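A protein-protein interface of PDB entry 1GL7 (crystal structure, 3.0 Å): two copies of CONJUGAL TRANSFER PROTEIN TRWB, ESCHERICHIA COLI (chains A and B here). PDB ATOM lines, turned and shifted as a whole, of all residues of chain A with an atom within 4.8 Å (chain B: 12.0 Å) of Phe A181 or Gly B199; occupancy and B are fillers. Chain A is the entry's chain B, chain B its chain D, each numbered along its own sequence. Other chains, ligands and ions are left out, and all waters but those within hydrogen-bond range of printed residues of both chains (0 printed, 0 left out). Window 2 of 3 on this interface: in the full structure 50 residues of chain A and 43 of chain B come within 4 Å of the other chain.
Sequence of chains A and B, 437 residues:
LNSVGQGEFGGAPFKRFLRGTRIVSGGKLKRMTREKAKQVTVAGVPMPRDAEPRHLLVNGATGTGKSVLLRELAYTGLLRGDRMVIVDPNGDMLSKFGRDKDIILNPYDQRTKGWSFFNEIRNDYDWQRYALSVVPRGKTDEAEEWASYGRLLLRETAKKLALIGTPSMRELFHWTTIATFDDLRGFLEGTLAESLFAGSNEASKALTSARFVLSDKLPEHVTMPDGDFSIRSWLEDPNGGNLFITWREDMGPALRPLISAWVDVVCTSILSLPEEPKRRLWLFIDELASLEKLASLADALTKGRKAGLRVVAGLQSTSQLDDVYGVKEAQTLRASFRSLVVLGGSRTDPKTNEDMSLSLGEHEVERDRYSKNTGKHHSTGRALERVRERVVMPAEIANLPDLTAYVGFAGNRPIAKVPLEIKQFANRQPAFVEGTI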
ATOM      1  N   ALA A 179      30.095  21.832  13.367  1.00  0.00           N
ATOM      2  CA  ALA A 179      30.885  22.633  14.296  1.00  0.00           C
ATOM      3  C   ALA A 179      29.943  23.580  15.030  1.00  0.00           C
ATOM      4  O   ALA A 179      28.861  23.883  14.547  1.00  0.00           O
ATOM      5  CB  ALA A 179      31.968  23.431  13.538  1.00  0.00           C
ATOM      6  N   THR A 180      30.338  24.035  16.210  1.00  0.00           N
ATOM      7  CA  THR A 180      29.489  24.961  16.947  1.00  0.00           C
ATOM      8  C   THR A 180      29.575  26.294  16.239  1.00  0.00           C
ATOM      9  O   THR A 180      30.476  26.530  15.429  1.00  0.00           O
ATOM     10  CB  THR A 180      29.974  25.216  18.370  1.00  0.00           C
ATOM     11  OG1 THR A 180      31.140  26.050  18.328  1.00  0.00           O
ATOM     12  CG2 THR A 180      30.316  23.919  19.052  1.00  0.00           C
ATOM     13  N   PHE A 181      28.642  27.170  16.577  1.00  0.00           N
ATOM     14  CA  PHE A 181      28.595  28.499  15.993  1.00  0.00           C
ATOM     15  C   PHE A 181      29.967  29.174  16.091  1.00  0.00           C
ATOM     16  O   PHE A 181      30.559  29.579  15.086  1.00  0.00           O
ATOM     17  CB  PHE A 181      27.560  29.340  16.746  1.00  0.00           C
ATOM     18  CG  PHE A 181      26.537  29.997  15.860  1.00  0.00           C
ATOM     19  CD1 PHE A 181      25.696  29.235  15.057  1.00  0.00           C
ATOM     20  CD2 PHE A 181      26.388  31.383  15.861  1.00  0.00           C
ATOM     21  CE1 PHE A 181      24.717  29.843  14.269  1.00  0.00           C
ATOM     22  CE2 PHE A 181      25.413  32.003  15.078  1.00  0.00           C
ATOM     23  CZ  PHE A 181      24.573  31.231  14.280  1.00  0.00           C
ATOM     24  N   ASP A 182      30.460  29.272  17.320  1.00  0.00           N
ATOM     25  CA  ASP A 182      31.727  29.914  17.601  1.00  0.00           C
ATOM     26  C   ASP A 182      32.890  29.307  16.843  1.00  0.00           C
ATOM     27  O   ASP A 182      33.660  30.026  16.212  1.00  0.00           O
ATOM     28  CB  ASP A 182      31.983  29.873  19.100  1.00  0.00           C
ATOM     29  CG  ASP A 182      30.791  30.373  19.902  1.00  0.00           C
ATOM     30  OD1 ASP A 182      30.989  31.238  20.785  1.00  0.00           O
ATOM     31  OD2 ASP A 182      29.655  29.902  19.652  1.00  0.00           O
ATOM     32  N   ASP A 183      33.020  27.990  16.898  1.00  0.00           N
ATOM     33  CA  ASP A 183      34.110  27.337  16.197  1.00  0.00           C
ATOM     34  C   ASP A 183      34.088  27.733  14.733  1.00  0.00           C
ATOM     35  O   ASP A 183      35.105  28.147  14.171  1.00  0.00           O
ATOM     36  CB  ASP A 183      33.988  25.823  16.320  1.00  0.00           C
ATOM     37  CG  ASP A 183      34.084  25.346  17.755  1.00  0.00           C
ATOM     38  OD1 ASP A 183      35.033  25.749  18.459  1.00  0.00           O
ATOM     39  OD2 ASP A 183      33.212  24.559  18.173  1.00  0.00           O
ATOM     40  N   LEU A 184      32.918  27.604  14.119  1.00  0.00           N
ATOM     41  CA  LEU A 184      32.764  27.961  12.717  1.00  0.00           C
ATOM     42  C   LEU A 184      33.238  29.404  12.570  1.00  0.00           C
ATOM     43  O   LEU A 184      34.143  29.698  11.777  1.00  0.00           O
ATOM     44  CB  LEU A 184      31.296  27.846  12.307  1.00  0.00           C
ATOM     45  CG  LEU A 184      31.021  27.408  10.865  1.00  0.00           C
ATOM     46  CD1 LEU A 184      29.527  27.548  10.575  1.00  0.00           C
ATOM     47  CD2 LEU A 184      31.851  28.242   9.892  1.00  0.00           C
ATOM     48  N   ARG A 185      32.620  30.294  13.342  1.00  0.00           N
ATOM     49  CA  ARG A 185      32.973  31.711  13.346  1.00  0.00           C
ATOM     50  C   ARG A 185      34.488  31.874  13.356  1.00  0.00           C
ATOM     51  O   ARG A 185      35.051  32.650  12.581  1.00  0.00           O
ATOM     52  CB  ARG A 185      32.392  32.389  14.584  1.00  0.00           C
ATOM     53  CG  ARG A 185      30.937  32.797  14.466  1.00  0.00           C
ATOM     54  CD  ARG A 185      30.814  34.317  14.260  1.00  0.00           C
ATOM     55  NE  ARG A 185      29.430  34.757  14.072  1.00  0.00           N
ATOM     56  CZ  ARG A 185      28.449  34.560  14.948  1.00  0.00           C
ATOM     57  NH1 ARG A 185      27.227  34.998  14.675  1.00  0.00           N
ATOM     58  NH2 ARG A 185      28.690  33.932  16.096  1.00  0.00           N
ATOM     59  N   SER A 204      23.526  36.813  12.936  1.00  0.00           N
ATOM     60  CA  SER A 204      23.459  35.447  13.468  1.00  0.00           C
ATOM     61  C   SER A 204      22.372  34.664  12.752  1.00  0.00           C
ATOM     62  O   SER A 204      22.567  33.523  12.342  1.00  0.00           O
ATOM     63  CB  SER A 204      23.140  35.469  14.964  1.00  0.00           C
ATOM     64  OG  SER A 204      23.976  36.380  15.655  1.00  0.00           O
ATOM     65  N   LEU A 207      23.382  33.515   9.482  1.00  0.00           N
ATOM     66  CA  LEU A 207      24.257  32.355   9.534  1.00  0.00           C
ATOM     67  C   LEU A 207      23.415  31.104   9.749  1.00  0.00           C
ATOM     68  O   LEU A 207      23.612  30.083   9.090  1.00  0.00           O
ATOM     69  CB  LEU A 207      25.263  32.482  10.678  1.00  0.00           C
ATOM     70  CG  LEU A 207      26.610  31.759  10.521  1.00  0.00           C
ATOM     71  CD1 LEU A 207      27.034  31.191  11.881  1.00  0.00           C
ATOM     72  CD2 LEU A 207      26.514  30.629   9.506  1.00  0.00           C
ATOM     73  N   THR A 208      22.477  31.187  10.685  1.00  0.00           N
ATOM     74  CA  THR A 208      21.597  30.066  10.982  1.00  0.00           C
ATOM     75  C   THR A 208      20.960  29.543   9.691  1.00  0.00           C
ATOM     76  O   THR A 208      20.988  28.339   9.398  1.00  0.00           O
ATOM     77  CB  THR A 208      20.477  30.492  11.951  1.00  0.00           C
ATOM     78  OG1 THR A 208      21.039  30.761  13.246  1.00  0.00           O
ATOM     79  CG2 THR A 208      19.417  29.391  12.061  1.00  0.00           C
ATOM     80  N   ARG A 211      23.249  27.629   7.410  1.00  0.00           N
ATOM     81  CA  ARG A 211      23.511  26.293   7.927  1.00  0.00           C
ATOM     82  C   ARG A 211      22.436  25.330   7.490  1.00  0.00           C
ATOM     83  O   ARG A 211      22.726  24.256   6.958  1.00  0.00           O
ATOM     84  CB  ARG A 211      23.566  26.318   9.445  1.00  0.00           C
ATOM     85  CG  ARG A 211      24.806  26.984   9.989  1.00  0.00           C
ATOM     86  CD  ARG A 211      25.896  25.961  10.353  1.00  0.00           C
ATOM     87  NE  ARG A 211      26.071  25.812  11.798  1.00  0.00           N
ATOM     88  CZ  ARG A 211      26.975  25.024  12.371  1.00  0.00           C
ATOM     89  NH1 ARG A 211      27.801  24.293  11.628  1.00  0.00           N
ATOM     90  NH2 ARG A 211      27.045  24.971  13.695  1.00  0.00           N
ATOM     91  N   PHE B 181      13.727  21.925  26.602  1.00  0.00           N
ATOM     92  CA  PHE B 181      14.593  22.336  25.513  1.00  0.00           C
ATOM     93  C   PHE B 181      15.992  21.764  25.683  1.00  0.00           C
ATOM     94  O   PHE B 181      16.522  21.105  24.796  1.00  0.00           O
ATOM     95  CB  PHE B 181      14.674  23.855  25.466  1.00  0.00           C
ATOM     96  CG  PHE B 181      14.136  24.454  24.205  1.00  0.00           C
ATOM     97  CD1 PHE B 181      12.791  24.319  23.864  1.00  0.00           C
ATOM     98  CD2 PHE B 181      14.979  25.147  23.353  1.00  0.00           C
ATOM     99  CE1 PHE B 181      12.297  24.884  22.694  1.00  0.00           C
ATOM    100  CE2 PHE B 181      14.499  25.716  22.186  1.00  0.00           C
ATOM    101  CZ  PHE B 181      13.155  25.580  21.852  1.00  0.00           C
ATOM    102  N   ASP B 182      16.571  22.020  26.849  1.00  0.00           N
ATOM    103  CA  ASP B 182      17.921  21.571  27.161  1.00  0.00           C
ATOM    104  C   ASP B 182      18.094  20.075  27.039  1.00  0.00           C
ATOM    105  O   ASP B 182      18.954  19.603  26.293  1.00  0.00           O
ATOM    106  CB  ASP B 182      18.304  21.997  28.575  1.00  0.00           C
ATOM    107  CG  ASP B 182      18.073  23.476  28.829  1.00  0.00           C
ATOM    108  OD1 ASP B 182      18.584  23.985  29.850  1.00  0.00           O
ATOM    109  OD2 ASP B 182      17.367  24.127  28.017  1.00  0.00           O
ATOM    110  N   ARG B 185      17.887  19.049  23.638  1.00  0.00           N
ATOM    111  CA  ARG B 185      19.130  19.550  23.089  1.00  0.00           C
ATOM    112  C   ARG B 185      20.248  18.558  23.393  1.00  0.00           C
ATOM    113  O   ARG B 185      21.033  18.191  22.520  1.00  0.00           O
ATOM    114  CB  ARG B 185      19.444  20.907  23.719  1.00  0.00           C
ATOM    115  CG  ARG B 185      18.744  22.105  23.083  1.00  0.00           C
ATOM    116  CD  ARG B 185      19.663  22.710  22.033  1.00  0.00           C
ATOM    117  NE  ARG B 185      19.236  24.013  21.536  1.00  0.00           N
ATOM    118  CZ  ARG B 185      18.954  25.055  22.308  1.00  0.00           C
ATOM    119  NH1 ARG B 185      18.586  26.200  21.756  1.00  0.00           N
ATOM    120  NH2 ARG B 185      19.018  24.945  23.628  1.00  0.00           N
ATOM    121  N   GLY B 186      20.306  18.119  24.641  1.00  0.00           N
ATOM    122  CA  GLY B 186      21.329  17.177  25.028  1.00  0.00           C
ATOM    123  C   GLY B 186      21.203  15.921  24.205  1.00  0.00           C
ATOM    124  O   GLY B 186      22.132  15.525  23.511  1.00  0.00           O
ATOM    125  N   LEU B 188      20.062  15.282  21.466  1.00  0.00           N
ATOM    126  CA  LEU B 188      20.429  15.423  20.060  1.00  0.00           C
ATOM    127  C   LEU B 188      21.910  15.497  19.790  1.00  0.00           C
ATOM    128  O   LEU B 188      22.334  15.408  18.637  1.00  0.00           O
ATOM    129  CB  LEU B 188      19.744  16.638  19.443  1.00  0.00           C
ATOM    130  CG  LEU B 188      18.260  16.392  19.153  1.00  0.00           C
ATOM    131  CD1 LEU B 188      17.619  17.662  18.678  1.00  0.00           C
ATOM    132  CD2 LEU B 188      18.108  15.301  18.105  1.00  0.00           C
ATOM    133  N   GLU B 189      22.702  15.667  20.842  1.00  0.00           N
ATOM    134  CA  GLU B 189      24.141  15.715  20.661  1.00  0.00           C
ATOM    135  C   GLU B 189      24.552  14.433  19.964  1.00  0.00           C
ATOM    136  O   GLU B 189      24.119  13.347  20.344  1.00  0.00           O
ATOM    137  CB  GLU B 189      24.849  15.784  21.998  1.00  0.00           C
ATOM    138  CG  GLU B 189      24.616  17.050  22.762  1.00  0.00           C
ATOM    139  CD  GLU B 189      25.281  16.991  24.114  1.00  0.00           C
ATOM    140  OE1 GLU B 189      26.468  16.595  24.162  1.00  0.00           O
ATOM    141  OE2 GLU B 189      24.624  17.335  25.124  1.00  0.00           O
ATOM    142  N   LEU B 192      22.929  14.592  13.543  1.00  0.00           N
ATOM    143  CA  LEU B 192      23.083  15.679  12.589  1.00  0.00           C
ATOM    144  C   LEU B 192      22.426  16.975  13.071  1.00  0.00           C
ATOM    145  O   LEU B 192      22.902  18.080  12.795  1.00  0.00           O
ATOM    146  CB  LEU B 192      22.472  15.245  11.268  1.00  0.00           C
ATOM    147  CG  LEU B 192      23.246  14.072  10.696  1.00  0.00           C
ATOM    148  CD1 LEU B 192      22.533  13.471   9.512  1.00  0.00           C
ATOM    149  CD2 LEU B 192      24.610  14.579  10.299  1.00  0.00           C
ATOM    150  N   ALA B 193      21.337  16.820  13.811  1.00  0.00           N
ATOM    151  CA  ALA B 193      20.576  17.945  14.331  1.00  0.00           C
ATOM    152  C   ALA B 193      21.227  18.638  15.521  1.00  0.00           C
ATOM    153  O   ALA B 193      20.789  19.710  15.939  1.00  0.00           O
ATOM    154  CB  ALA B 193      19.198  17.469  14.717  1.00  0.00           C
ATOM    155  N   GLU B 194      22.268  18.027  16.071  1.00  0.00           N
ATOM    156  CA  GLU B 194      22.938  18.610  17.220  1.00  0.00           C
ATOM    157  C   GLU B 194      23.139  20.111  17.089  1.00  0.00           C
ATOM    158  O   GLU B 194      22.526  20.887  17.817  1.00  0.00           O
ATOM    159  CB  GLU B 194      24.291  17.948  17.464  1.00  0.00           C
ATOM    160  CG  GLU B 194      24.990  18.488  18.707  1.00  0.00           C
ATOM    161  CD  GLU B 194      26.303  17.795  18.992  1.00  0.00           C
ATOM    162  OE1 GLU B 194      26.958  18.182  19.983  1.00  0.00           O
ATOM    163  OE2 GLU B 194      26.676  16.869  18.232  1.00  0.00           O
ATOM    164  N   SER B 195      23.978  20.532  16.154  1.00  0.00           N
ATOM    165  CA  SER B 195      24.231  21.954  16.005  1.00  0.00           C
ATOM    166  C   SER B 195      23.106  22.795  15.408  1.00  0.00           C
ATOM    167  O   SER B 195      22.715  23.789  16.005  1.00  0.00           O
ATOM    168  CB  SER B 195      25.526  22.177  15.213  1.00  0.00           C
ATOM    169  OG  SER B 195      26.668  21.978  16.034  1.00  0.00           O
ATOM    170  N   LEU B 196      22.585  22.387  14.251  1.00  0.00           N
ATOM    171  CA  LEU B 196      21.528  23.130  13.533  1.00  0.00           C
ATOM    172  C   LEU B 196      20.442  23.826  14.367  1.00  0.00           C
ATOM    173  O   LEU B 196      19.936  24.892  13.976  1.00  0.00           O
ATOM    174  CB  LEU B 196      20.835  22.217  12.514  1.00  0.00           C
ATOM    175  CG  LEU B 196      21.702  21.488  11.495  1.00  0.00           C
ATOM    176  CD1 LEU B 196      20.891  20.349  10.929  1.00  0.00           C
ATOM    177  CD2 LEU B 196      22.174  22.432  10.415  1.00  0.00           C
ATOM    178  N   PHE B 197      20.074  23.232  15.501  1.00  0.00           N
ATOM    179  CA  PHE B 197      19.024  23.812  16.333  1.00  0.00           C
ATOM    180  C   PHE B 197      19.515  24.648  17.494  1.00  0.00           C
ATOM    181  O   PHE B 197      18.797  24.850  18.462  1.00  0.00           O
ATOM    182  CB  PHE B 197      18.111  22.712  16.863  1.00  0.00           C
ATOM    183  CG  PHE B 197      17.053  22.278  15.893  1.00  0.00           C
ATOM    184  CD1 PHE B 197      17.011  20.965  15.442  1.00  0.00           C
ATOM    185  CD2 PHE B 197      16.073  23.177  15.463  1.00  0.00           C
ATOM    186  CE1 PHE B 197      16.005  20.536  14.578  1.00  0.00           C
ATOM    187  CE2 PHE B 197      15.054  22.770  14.598  1.00  0.00           C
ATOM    188  CZ  PHE B 197      15.018  21.444  14.152  1.00  0.00           C
ATOM    189  N   ALA B 198      20.735  25.146  17.404  1.00  0.00           N
ATOM    190  CA  ALA B 198      21.264  25.948  18.490  1.00  0.00           C
ATOM    191  C   ALA B 198      22.239  26.995  17.960  1.00  0.00           C
ATOM    192  O   ALA B 198      22.810  26.819  16.880  1.00  0.00           O
ATOM    193  CB  ALA B 198      21.950  25.040  19.498  1.00  0.00           C
ATOM    194  N   GLY B 199      22.414  28.091  18.702  1.00  0.00           N
ATOM    195  CA  GLY B 199      23.343  29.128  18.272  1.00  0.00           C
ATOM    196  C   GLY B 199      22.826  30.556  18.139  1.00  0.00           C
ATOM    197  O   GLY B 199      23.597  31.503  18.290  1.00  0.00           O
ATOM    198  N   SER B 200      21.544  30.728  17.827  1.00  0.00           N
ATOM    199  CA  SER B 200      20.970  32.066  17.690  1.00  0.00           C
ATOM    200  C   SER B 200      19.511  31.952  18.062  1.00  0.00           C
ATOM    201  O   SER B 200      19.027  30.856  18.340  1.00  0.00           O
ATOM    202  CB  SER B 200      21.072  32.562  16.246  1.00  0.00           C
ATOM    203  OG  SER B 200      20.150  31.868  15.424  1.00  0.00           O
ATOM    204  N   ASN B 201      18.802  33.074  18.065  1.00  0.00           N
ATOM    205  CA  ASN B 201      17.381  33.040  18.401  1.00  0.00           C
ATOM    206  C   ASN B 201      16.622  32.326  17.284  1.00  0.00           C
ATOM    207  O   ASN B 201      15.640  31.609  17.531  1.00  0.00           O
ATOM    208  CB  ASN B 201      16.844  34.457  18.598  1.00  0.00           C
ATOM    209  CG  ASN B 201      17.533  35.180  19.743  1.00  0.00           C
ATOM    210  OD1 ASN B 201      17.225  34.950  20.919  1.00  0.00           O
ATOM    211  ND2 ASN B 201      18.485  36.050  19.405  1.00  0.00           N
ATOM    212  N   GLU B 202      17.088  32.527  16.055  1.00  0.00           N
ATOM    213  CA  GLU B 202      16.479  31.882  14.905  1.00  0.00           C
ATOM    214  C   GLU B 202      16.503  30.379  15.171  1.00  0.00           C
ATOM    215  O   GLU B 202      15.468  29.716  15.133  1.00  0.00           O
ATOM    216  CB  GLU B 202      17.271  32.199  13.636  1.00  0.00           C
ATOM    217  CG  GLU B 202      16.587  31.728  12.370  1.00  0.00           C
ATOM    218  CD  GLU B 202      15.201  32.324  12.197  1.00  0.00           C
ATOM    219  OE1 GLU B 202      14.531  31.991  11.198  1.00  0.00           O
ATOM    220  OE2 GLU B 202      14.780  33.129  13.057  1.00  0.00           O
ATOM    221  N   ALA B 203      17.697  29.856  15.457  1.00  0.00           N
ATOM    222  CA  ALA B 203      17.873  28.441  15.756  1.00  0.00           C
ATOM    223  C   ALA B 203      16.828  27.975  16.780  1.00  0.00           C
ATOM    224  O   ALA B 203      16.147  26.980  16.565  1.00  0.00           O
ATOM    225  CB  ALA B 203      19.290  28.198  16.281  1.00  0.00           C
ATOM    226  N   SER B 204      16.686  28.701  17.884  1.00  0.00           N
ATOM    227  CA  SER B 204      15.712  28.326  18.907  1.00  0.00           C
ATOM    228  C   SER B 204      14.322  28.342  18.332  1.00  0.00           C
ATOM    229  O   SER B 204      13.537  27.417  18.530  1.00  0.00           O
ATOM    230  CB  SER B 204      15.755  29.304  20.069  1.00  0.00           C
ATOM    231  OG  SER B 204      17.030  29.276  20.666  1.00  0.00           O
ATOM    232  N   LYS B 205      14.017  29.421  17.632  1.00  0.00           N
ATOM    233  CA  LYS B 205      12.714  29.586  17.022  1.00  0.00           C
ATOM    234  C   LYS B 205      12.383  28.387  16.149  1.00  0.00           C
ATOM    235  O   LYS B 205      11.265  27.874  16.165  1.00  0.00           O
ATOM    236  CB  LYS B 205      12.715  30.858  16.182  1.00  0.00           C
ATOM    237  CG  LYS B 205      11.417  31.146  15.446  1.00  0.00           C
ATOM    238  CD  LYS B 205      11.649  32.267  14.430  1.00  0.00           C
ATOM    239  CE  LYS B 205      10.500  32.399  13.445  1.00  0.00           C
ATOM    240  NZ  LYS B 205      10.839  33.386  12.376  1.00  0.00           N
ATOM    241  N   ALA B 206      13.371  27.949  15.384  1.00  0.00           N
ATOM    242  CA  ALA B 206      13.202  26.809  14.494  1.00  0.00           C
ATOM    243  C   ALA B 206      12.785  25.577  15.281  1.00  0.00           C
ATOM    244  O   ALA B 206      11.861  24.864  14.895  1.00  0.00           O
ATOM    245  CB  ALA B 206      14.500  26.535  13.744  1.00  0.00           C
ATOM    246  N   LEU B 207      13.475  25.334  16.384  1.00  0.00           N
ATOM    247  CA  LEU B 207      13.173  24.185  17.206  1.00  0.00           C
ATOM    248  C   LEU B 207      11.743  24.259  17.722  1.00  0.00           C
ATOM    249  O   LEU B 207      10.996  23.280  17.651  1.00  0.00           O
ATOM    250  CB  LEU B 207      14.130  24.117  18.391  1.00  0.00           C
ATOM    251  CG  LEU B 207      14.513  22.699  18.838  1.00  0.00           C
ATOM    252  CD1 LEU B 207      14.954  22.708  20.300  1.00  0.00           C
ATOM    253  CD2 LEU B 207      13.326  21.765  18.651  1.00  0.00           C
ATOM    254  N   THR B 208      11.363  25.421  18.248  1.00  0.00           N
ATOM    255  CA  THR B 208      10.014  25.617  18.783  1.00  0.00           C
ATOM    256  C   THR B 208       8.990  25.208  17.729  1.00  0.00           C
ATOM    257  O   THR B 208       8.009  24.516  18.029  1.00  0.00           O
ATOM    258  CB  THR B 208       9.766  27.090  19.161  1.00  0.00           C
ATOM    259  OG1 THR B 208      10.715  27.495  20.154  1.00  0.00           O
ATOM    260  CG2 THR B 208       8.361  27.262  19.708  1.00  0.00           C
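The backbone carbonyl oxygen (O) of Ala A179 is in hydrogen-bond range of the side-chain hydroxyl (OG) of Ser B195, at 3.3 Å. The side-chain hydroxyl (OG1) of Thr A208 sits at hydrogen-bond distance from the side-chain hydroxyl (OG) of Ser B200 (2.6 Å).
O of Ala A179 lies close to NH1 of Arg A211. The side-chain hydroxyl (OG1) of Thr A208 is in hydrogen-bond range of the backbone carbonyl oxygen (O) of Ser A204 (3.3 Å). The backbone NH (N) of Glu B202 sits at hydrogen-bond distance from the side-chain hydroxyl (OG) of Ser B200, at 3.2 Å. OG of Ser B200 sits at hydrogen-bond distance from N of Ala B203 (3.2 Å). OG of Ser B204 lies within hydrogen-bond range of O of Ser B200 (3.4 Å).
Among the printed residues, pairs that only touch across the chains: Phe A181 with Gly B199, Ser A204 with Ser B200, Thr A208 with Glu B202, Thr A208 with Ala B203, Arg A211 with Ser B195 and Arg A211 with Leu B196.
No residue of chain B comes within 4 Å of Thr A180. Phe A181 touches one residue of chain B. No residue of chain B comes within 4 Å of Asp A182. No residue of chain B comes within 4 Å of Asp A183. No residue of chain B comes within 4 Å of Leu A184. No residue of chain B comes within 4 Å of Arg A185. Of chain B, only Ser B200 (3.8 Å) comes within 4 Å of Ser A204. Thr A208 touches just these residues of chain B: Ser B200, Glu B202 and Ala B203. Of the printed residues of chain A, Ser B195 touches Ala A179 (3.3 Å) and Arg A211 (3.5 Å). Of the printed residues of chain A, Gly B199 touches Phe A181. Printed residues of chain A within 4 Å of Ser B200: Ser A204 (3.8 Å) and Thr A208 (2.6 Å). Ser B204 touches none of the printed residues of chain A. The nearest printed residue of chain A that does not touch Ala B203 is Phe A181 (6.0 Å).
Printed residues of chain A that touch a printed residue of chain B: Ala A179, Phe A181, Ser A204, Thr A208 and Arg A211. Hydrophobic or aromatic side chains of chain B that line the printed part of chain A: Leu B196. Among the printed residues, 8 pairs touch across the chains.
6 positions are printed for both chains. Of the 8 pairs that touch across the chains among the printed residues, none has its exchanged pair printed and touching as well.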
